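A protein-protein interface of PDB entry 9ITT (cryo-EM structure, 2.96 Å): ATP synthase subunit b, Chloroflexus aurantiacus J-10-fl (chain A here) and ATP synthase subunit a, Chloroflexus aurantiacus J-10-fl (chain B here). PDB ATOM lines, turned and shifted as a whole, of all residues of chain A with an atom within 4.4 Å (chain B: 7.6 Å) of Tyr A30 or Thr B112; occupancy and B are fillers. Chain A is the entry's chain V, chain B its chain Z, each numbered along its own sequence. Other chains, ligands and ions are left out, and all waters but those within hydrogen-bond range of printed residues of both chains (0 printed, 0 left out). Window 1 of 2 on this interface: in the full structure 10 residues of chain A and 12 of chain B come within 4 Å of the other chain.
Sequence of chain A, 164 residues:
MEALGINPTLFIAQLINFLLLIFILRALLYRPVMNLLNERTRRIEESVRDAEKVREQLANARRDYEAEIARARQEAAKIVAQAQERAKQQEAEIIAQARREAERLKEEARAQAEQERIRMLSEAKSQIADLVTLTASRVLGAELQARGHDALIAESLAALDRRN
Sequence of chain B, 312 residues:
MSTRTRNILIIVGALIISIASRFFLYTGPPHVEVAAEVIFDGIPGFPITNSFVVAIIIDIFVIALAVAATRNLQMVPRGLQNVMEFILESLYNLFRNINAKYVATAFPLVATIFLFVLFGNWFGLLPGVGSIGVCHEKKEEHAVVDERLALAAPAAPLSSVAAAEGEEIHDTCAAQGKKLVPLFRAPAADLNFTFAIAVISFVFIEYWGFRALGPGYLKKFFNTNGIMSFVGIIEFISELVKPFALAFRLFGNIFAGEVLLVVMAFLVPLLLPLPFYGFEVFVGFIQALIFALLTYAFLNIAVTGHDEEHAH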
ATOM      1  N   LEU A  25      17.546 -12.103  -2.853  1.00  0.00           N
ATOM      2  CA  LEU A  25      18.400 -11.059  -3.408  1.00  0.00           C
ATOM      3  C   LEU A  25      18.425  -9.839  -2.499  1.00  0.00           C
ATOM      4  O   LEU A  25      19.490  -9.263  -2.255  1.00  0.00           O
ATOM      5  CB  LEU A  25      17.930 -10.653  -4.808  1.00  0.00           C
ATOM      6  CG  LEU A  25      18.355 -11.466  -6.042  1.00  0.00           C
ATOM      7  CD1 LEU A  25      19.870 -11.505  -6.180  1.00  0.00           C
ATOM      8  CD2 LEU A  25      17.775 -12.866  -6.064  1.00  0.00           C
ATOM      9  N   ARG A  26      17.263  -9.438  -1.979  1.00  0.00           N
ATOM     10  CA  ARG A  26      17.184  -8.284  -1.097  1.00  0.00           C
ATOM     11  C   ARG A  26      18.025  -8.496   0.152  1.00  0.00           C
ATOM     12  O   ARG A  26      18.927  -7.702   0.433  1.00  0.00           O
ATOM     13  CB  ARG A  26      15.716  -8.035  -0.750  1.00  0.00           C
ATOM     14  CG  ARG A  26      15.406  -6.853   0.142  1.00  0.00           C
ATOM     15  CD  ARG A  26      13.898  -6.635   0.129  1.00  0.00           C
ATOM     16  NE  ARG A  26      13.435  -5.610   1.059  1.00  0.00           N
ATOM     17  CZ  ARG A  26      13.075  -5.829   2.317  1.00  0.00           C
ATOM     18  NH1 ARG A  26      13.180  -7.026   2.876  1.00  0.00           N
ATOM     19  NH2 ARG A  26      12.588  -4.821   3.035  1.00  0.00           N
ATOM     20  N   LEU A  28      20.459 -10.575   0.745  1.00  0.00           N
ATOM     21  CA  LEU A  28      21.881 -10.813   0.528  1.00  0.00           C
ATOM     22  C   LEU A  28      22.613  -9.626  -0.089  1.00  0.00           C
ATOM     23  O   LEU A  28      23.834  -9.524   0.072  1.00  0.00           O
ATOM     24  CB  LEU A  28      22.078 -12.047  -0.360  1.00  0.00           C
ATOM     25  CG  LEU A  28      22.115 -13.408   0.346  1.00  0.00           C
ATOM     26  CD1 LEU A  28      23.412 -13.578   1.132  1.00  0.00           C
ATOM     27  CD2 LEU A  28      20.912 -13.608   1.262  1.00  0.00           C
ATOM     28  N   LEU A  29      21.910  -8.734  -0.792  1.00  0.00           N
ATOM     29  CA  LEU A  29      22.537  -7.615  -1.486  1.00  0.00           C
ATOM     30  C   LEU A  29      22.040  -6.262  -1.009  1.00  0.00           C
ATOM     31  O   LEU A  29      22.843  -5.424  -0.583  1.00  0.00           O
ATOM     32  CB  LEU A  29      22.276  -7.740  -2.995  1.00  0.00           C
ATOM     33  CG  LEU A  29      22.968  -6.733  -3.920  1.00  0.00           C
ATOM     34  CD1 LEU A  29      24.485  -6.809  -3.782  1.00  0.00           C
ATOM     35  CD2 LEU A  29      22.549  -6.953  -5.368  1.00  0.00           C
ATOM     36  N   TYR A  30      20.727  -6.033  -1.050  1.00  0.00           N
ATOM     37  CA  TYR A  30      20.214  -4.668  -1.028  1.00  0.00           C
ATOM     38  C   TYR A  30      20.406  -4.027   0.336  1.00  0.00           C
ATOM     39  O   TYR A  30      20.668  -2.825   0.425  1.00  0.00           O
ATOM     40  CB  TYR A  30      18.736  -4.655  -1.424  1.00  0.00           C
ATOM     41  CG  TYR A  30      18.449  -4.958  -2.888  1.00  0.00           C
ATOM     42  CD1 TYR A  30      19.450  -5.394  -3.755  1.00  0.00           C
ATOM     43  CD2 TYR A  30      17.169  -4.803  -3.402  1.00  0.00           C
ATOM     44  CE1 TYR A  30      19.182  -5.665  -5.075  1.00  0.00           C
ATOM     45  CE2 TYR A  30      16.894  -5.071  -4.728  1.00  0.00           C
ATOM     46  CZ  TYR A  30      17.906  -5.502  -5.558  1.00  0.00           C
ATOM     47  OH  TYR A  30      17.646  -5.773  -6.877  1.00  0.00           O
ATOM     48  N   ARG A  31      20.277  -4.803   1.405  1.00  0.00           N
ATOM     49  CA  ARG A  31      20.497  -4.245   2.732  1.00  0.00           C
ATOM     50  C   ARG A  31      21.993  -4.041   2.952  1.00  0.00           C
ATOM     51  O   ARG A  31      22.391  -3.014   3.514  1.00  0.00           O
ATOM     52  CB  ARG A  31      19.868  -5.137   3.811  1.00  0.00           C
ATOM     53  CG  ARG A  31      18.330  -5.176   3.787  1.00  0.00           C
ATOM     54  CD  ARG A  31      17.725  -3.786   3.959  1.00  0.00           C
ATOM     55  NE  ARG A  31      16.281  -3.787   4.167  1.00  0.00           N
ATOM     56  CZ  ARG A  31      15.681  -3.873   5.348  1.00  0.00           C
ATOM     57  NH1 ARG A  31      16.367  -4.045   6.468  1.00  0.00           N
ATOM     58  NH2 ARG A  31      14.356  -3.782   5.409  1.00  0.00           N
ATOM     59  N   PRO A  32      22.856  -4.972   2.533  1.00  0.00           N
ATOM     60  CA  PRO A  32      24.279  -4.613   2.410  1.00  0.00           C
ATOM     61  C   PRO A  32      24.521  -3.428   1.488  1.00  0.00           C
ATOM     62  O   PRO A  32      25.343  -2.559   1.803  1.00  0.00           O
ATOM     63  CB  PRO A  32      24.911  -5.898   1.863  1.00  0.00           C
ATOM     64  CG  PRO A  32      24.067  -6.980   2.413  1.00  0.00           C
ATOM     65  CD  PRO A  32      22.662  -6.434   2.498  1.00  0.00           C
ATOM     66  N   VAL A  33      23.801  -3.333   0.368  1.00  0.00           N
ATOM     67  CA  VAL A  33      24.027  -2.212  -0.537  1.00  0.00           C
ATOM     68  C   VAL A  33      23.321  -0.944  -0.063  1.00  0.00           C
ATOM     69  O   VAL A  33      23.783   0.163  -0.374  1.00  0.00           O
ATOM     70  CB  VAL A  33      23.608  -2.565  -1.975  1.00  0.00           C
ATOM     71  CG1 VAL A  33      23.731  -1.351  -2.873  1.00  0.00           C
ATOM     72  CG2 VAL A  33      24.493  -3.673  -2.526  1.00  0.00           C
ATOM     73  N   MET A  34      22.234  -1.056   0.706  1.00  0.00           N
ATOM     74  CA  MET A  34      21.717   0.146   1.349  1.00  0.00           C
ATOM     75  C   MET A  34      22.684   0.615   2.422  1.00  0.00           C
ATOM     76  O   MET A  34      22.850   1.822   2.622  1.00  0.00           O
ATOM     77  CB  MET A  34      20.312  -0.083   1.927  1.00  0.00           C
ATOM     78  CG  MET A  34      20.213  -0.436   3.418  1.00  0.00           C
ATOM     79  SD  MET A  34      18.494  -0.559   3.942  1.00  0.00           S
ATOM     80  CE  MET A  34      18.086   1.169   4.174  1.00  0.00           C
ATOM     81  N   VAL B  62      22.267 -13.728 -10.343  1.00  0.00           N
ATOM     82  CA  VAL B  62      22.287 -12.424  -9.691  1.00  0.00           C
ATOM     83  C   VAL B  62      22.629 -12.588  -8.215  1.00  0.00           C
ATOM     84  O   VAL B  62      23.251 -11.710  -7.614  1.00  0.00           O
ATOM     85  CB  VAL B  62      20.948 -11.685  -9.896  1.00  0.00           C
ATOM     86  N   ALA B  66      25.706 -10.765  -6.584  1.00  0.00           N
ATOM     87  CA  ALA B  66      25.511  -9.997  -5.362  1.00  0.00           C
ATOM     88  C   ALA B  66      26.521 -10.387  -4.295  1.00  0.00           C
ATOM     89  O   ALA B  66      27.157  -9.521  -3.684  1.00  0.00           O
ATOM     90  CB  ALA B  66      24.092 -10.216  -4.844  1.00  0.00           C
ATOM     91  N   THR B  70      29.056  -8.119  -2.472  1.00  0.00           N
ATOM     92  CA  THR B  70      29.080  -7.974  -1.021  1.00  0.00           C
ATOM     93  C   THR B  70      30.179  -8.796  -0.359  1.00  0.00           C
ATOM     94  O   THR B  70      30.245  -8.828   0.875  1.00  0.00           O
ATOM     95  CB  THR B  70      27.721  -8.359  -0.425  1.00  0.00           C
ATOM     96  N   LEU B  88      22.846   1.403  -8.284  1.00  0.00           N
ATOM     97  CA  LEU B  88      21.899   1.601  -7.193  1.00  0.00           C
ATOM     98  C   LEU B  88      21.733   3.079  -6.854  1.00  0.00           C
ATOM     99  O   LEU B  88      20.607   3.554  -6.676  1.00  0.00           O
ATOM    100  CB  LEU B  88      22.341   0.807  -5.963  1.00  0.00           C
ATOM    101  N   ALA B 106       9.450   1.662  -1.532  1.00  0.00           N
ATOM    102  CA  ALA B 106       9.338   0.946  -2.794  1.00  0.00           C
ATOM    103  C   ALA B 106      10.685   0.671  -3.450  1.00  0.00           C
ATOM    104  O   ALA B 106      10.721   0.030  -4.505  1.00  0.00           O
ATOM    105  CB  ALA B 106       8.452   1.733  -3.763  1.00  0.00           C
ATOM    106  N   PHE B 107      11.787   1.144  -2.862  1.00  0.00           N
ATOM    107  CA  PHE B 107      13.095   0.947  -3.484  1.00  0.00           C
ATOM    108  C   PHE B 107      13.439  -0.522  -3.683  1.00  0.00           C
ATOM    109  O   PHE B 107      13.920  -0.871  -4.774  1.00  0.00           O
ATOM    110  CB  PHE B 107      14.178   1.657  -2.663  1.00  0.00           C
ATOM    111  N   PRO B 108      13.242  -1.423  -2.710  1.00  0.00           N
ATOM    112  CA  PRO B 108      13.608  -2.828  -2.964  1.00  0.00           C
ATOM    113  C   PRO B 108      12.833  -3.453  -4.110  1.00  0.00           C
ATOM    114  O   PRO B 108      13.437  -4.065  -5.000  1.00  0.00           O
ATOM    115  CB  PRO B 108      13.300  -3.519  -1.626  1.00  0.00           C
ATOM    116  N   LEU B 109      11.504  -3.309  -4.111  1.00  0.00           N
ATOM    117  CA  LEU B 109      10.686  -3.884  -5.174  1.00  0.00           C
ATOM    118  C   LEU B 109      11.053  -3.287  -6.527  1.00  0.00           C
ATOM    119  O   LEU B 109      11.203  -4.010  -7.521  1.00  0.00           O
ATOM    120  CB  LEU B 109       9.204  -3.654  -4.865  1.00  0.00           C
ATOM    121  N   VAL B 110      11.214  -1.965  -6.582  1.00  0.00           N
ATOM    122  CA  VAL B 110      11.528  -1.307  -7.846  1.00  0.00           C
ATOM    123  C   VAL B 110      12.882  -1.781  -8.366  1.00  0.00           C
ATOM    124  O   VAL B 110      13.030  -2.129  -9.546  1.00  0.00           O
ATOM    125  CB  VAL B 110      11.485   0.222  -7.668  1.00  0.00           C
ATOM    126  N   ALA B 111      13.887  -1.816  -7.488  1.00  0.00           N
ATOM    127  CA  ALA B 111      15.234  -2.179  -7.910  1.00  0.00           C
ATOM    128  C   ALA B 111      15.300  -3.632  -8.359  1.00  0.00           C
ATOM    129  O   ALA B 111      15.934  -3.949  -9.372  1.00  0.00           O
ATOM    130  CB  ALA B 111      16.224  -1.920  -6.773  1.00  0.00           C
ATOM    131  N   THR B 112      14.664  -4.540  -7.610  1.00  0.00           N
ATOM    132  CA  THR B 112      14.703  -5.940  -8.016  1.00  0.00           C
ATOM    133  C   THR B 112      13.941  -6.160  -9.314  1.00  0.00           C
ATOM    134  O   THR B 112      14.398  -6.930 -10.166  1.00  0.00           O
ATOM    135  CB  THR B 112      14.167  -6.851  -6.904  1.00  0.00           C
ATOM    136  N   ILE B 113      12.803  -5.482  -9.501  1.00  0.00           N
ATOM    137  CA  ILE B 113      12.088  -5.590 -10.769  1.00  0.00           C
ATOM    138  C   ILE B 113      12.993  -5.149 -11.911  1.00  0.00           C
ATOM    139  O   ILE B 113      13.161  -5.863 -12.907  1.00  0.00           O
ATOM    140  CB  ILE B 113      10.788  -4.766 -10.725  1.00  0.00           C
ATOM    141  N   PHE B 114      13.617  -3.976 -11.764  1.00  0.00           N
ATOM    142  CA  PHE B 114      14.473  -3.456 -12.824  1.00  0.00           C
ATOM    143  C   PHE B 114      15.615  -4.416 -13.132  1.00  0.00           C
ATOM    144  O   PHE B 114      15.847  -4.769 -14.293  1.00  0.00           O
ATOM    145  CB  PHE B 114      15.032  -2.089 -12.433  1.00  0.00           C
ATOM    146  N   LEU B 115      16.341  -4.847 -12.099  1.00  0.00           N
ATOM    147  CA  LEU B 115      17.532  -5.657 -12.330  1.00  0.00           C
ATOM    148  C   LEU B 115      17.177  -7.021 -12.909  1.00  0.00           C
ATOM    149  O   LEU B 115      17.826  -7.485 -13.856  1.00  0.00           O
ATOM    150  CB  LEU B 115      18.325  -5.805 -11.030  1.00  0.00           C
ATOM    151  N   PHE B 116      16.154  -7.685 -12.362  1.00  0.00           N
ATOM    152  CA  PHE B 116      15.790  -8.990 -12.896  1.00  0.00           C
ATOM    153  C   PHE B 116      15.278  -8.882 -14.324  1.00  0.00           C
ATOM    154  O   PHE B 116      15.613  -9.721 -15.166  1.00  0.00           O
ATOM    155  CB  PHE B 116      14.746  -9.669 -12.016  1.00  0.00           C
ATOM    156  N   VAL B 117      14.460  -7.868 -14.622  1.00  0.00           N
ATOM    157  CA  VAL B 117      13.970  -7.716 -15.987  1.00  0.00           C
ATOM    158  C   VAL B 117      15.131  -7.447 -16.936  1.00  0.00           C
ATOM    159  O   VAL B 117      15.198  -8.017 -18.031  1.00  0.00           O
ATOM    160  CB  VAL B 117      12.906  -6.603 -16.053  1.00  0.00           C
ATOM    161  N   LEU B 118      16.067  -6.586 -16.529  1.00  0.00           N
ATOM    162  CA  LEU B 118      17.228  -6.291 -17.362  1.00  0.00           C
ATOM    163  C   LEU B 118      18.031  -7.552 -17.651  1.00  0.00           C
ATOM    164  O   LEU B 118      18.374  -7.834 -18.806  1.00  0.00           O
ATOM    165  CB  LEU B 118      18.100  -5.243 -16.663  1.00  0.00           C
ATOM    166  N   ALA B 292      10.319  -0.117 -14.026  1.00  0.00           N
ATOM    167  CA  ALA B 292      10.548   0.435 -12.695  1.00  0.00           C
ATOM    168  C   ALA B 292      10.100   1.889 -12.608  1.00  0.00           C
ATOM    169  O   ALA B 292       9.461   2.296 -11.627  1.00  0.00           O
ATOM    170  CB  ALA B 292      12.030   0.312 -12.345  1.00  0.00           C
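The backbone NH (N) of Arg A31 is in hydrogen-bond range of the backbone carbonyl oxygen (O) of Arg A26 (3.3 Å).
Of the printed residues of chain B, Arg A26 touches Pro B108 (3.4 Å). Tyr A30 touches just these residues of chain B: Pro B108, Ala B111 and Thr B112. Printed residues of chain A within 4 Å of Val B62: Leu A25 (3.6 Å). Of the printed residues of chain A, Ala B66 touches Leu A29. Of the printed residues of chain A, Pro B108 touches Arg A26 (3.4 Å) and Tyr A30 (3.6 Å). Thr B112 touches one residue of chain A. The nearest printed residue of chain A that does not touch Thr B112 is Leu A25 (5.7 Å).
Among the printed residues, merely in contact across the chains: Leu A25 with Val B62 (3.6 Å), Arg A26 with Pro B108 (3.4 Å), Leu A29 with Ala B66 (3.6 Å), Tyr A30 with Pro B108 (3.6 Å) and Tyr A30 with Ala B111 (3.5 Å).
Of the 9 printed residues of chain A, 4 touch a printed residue of chain B. Among the printed residues, 6 pairs touch across the chains.
The side-chain hydroxyl (OH) of Tyr A30 sits close to the backbone NH (N) of Thr B112 (3.3 Å).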
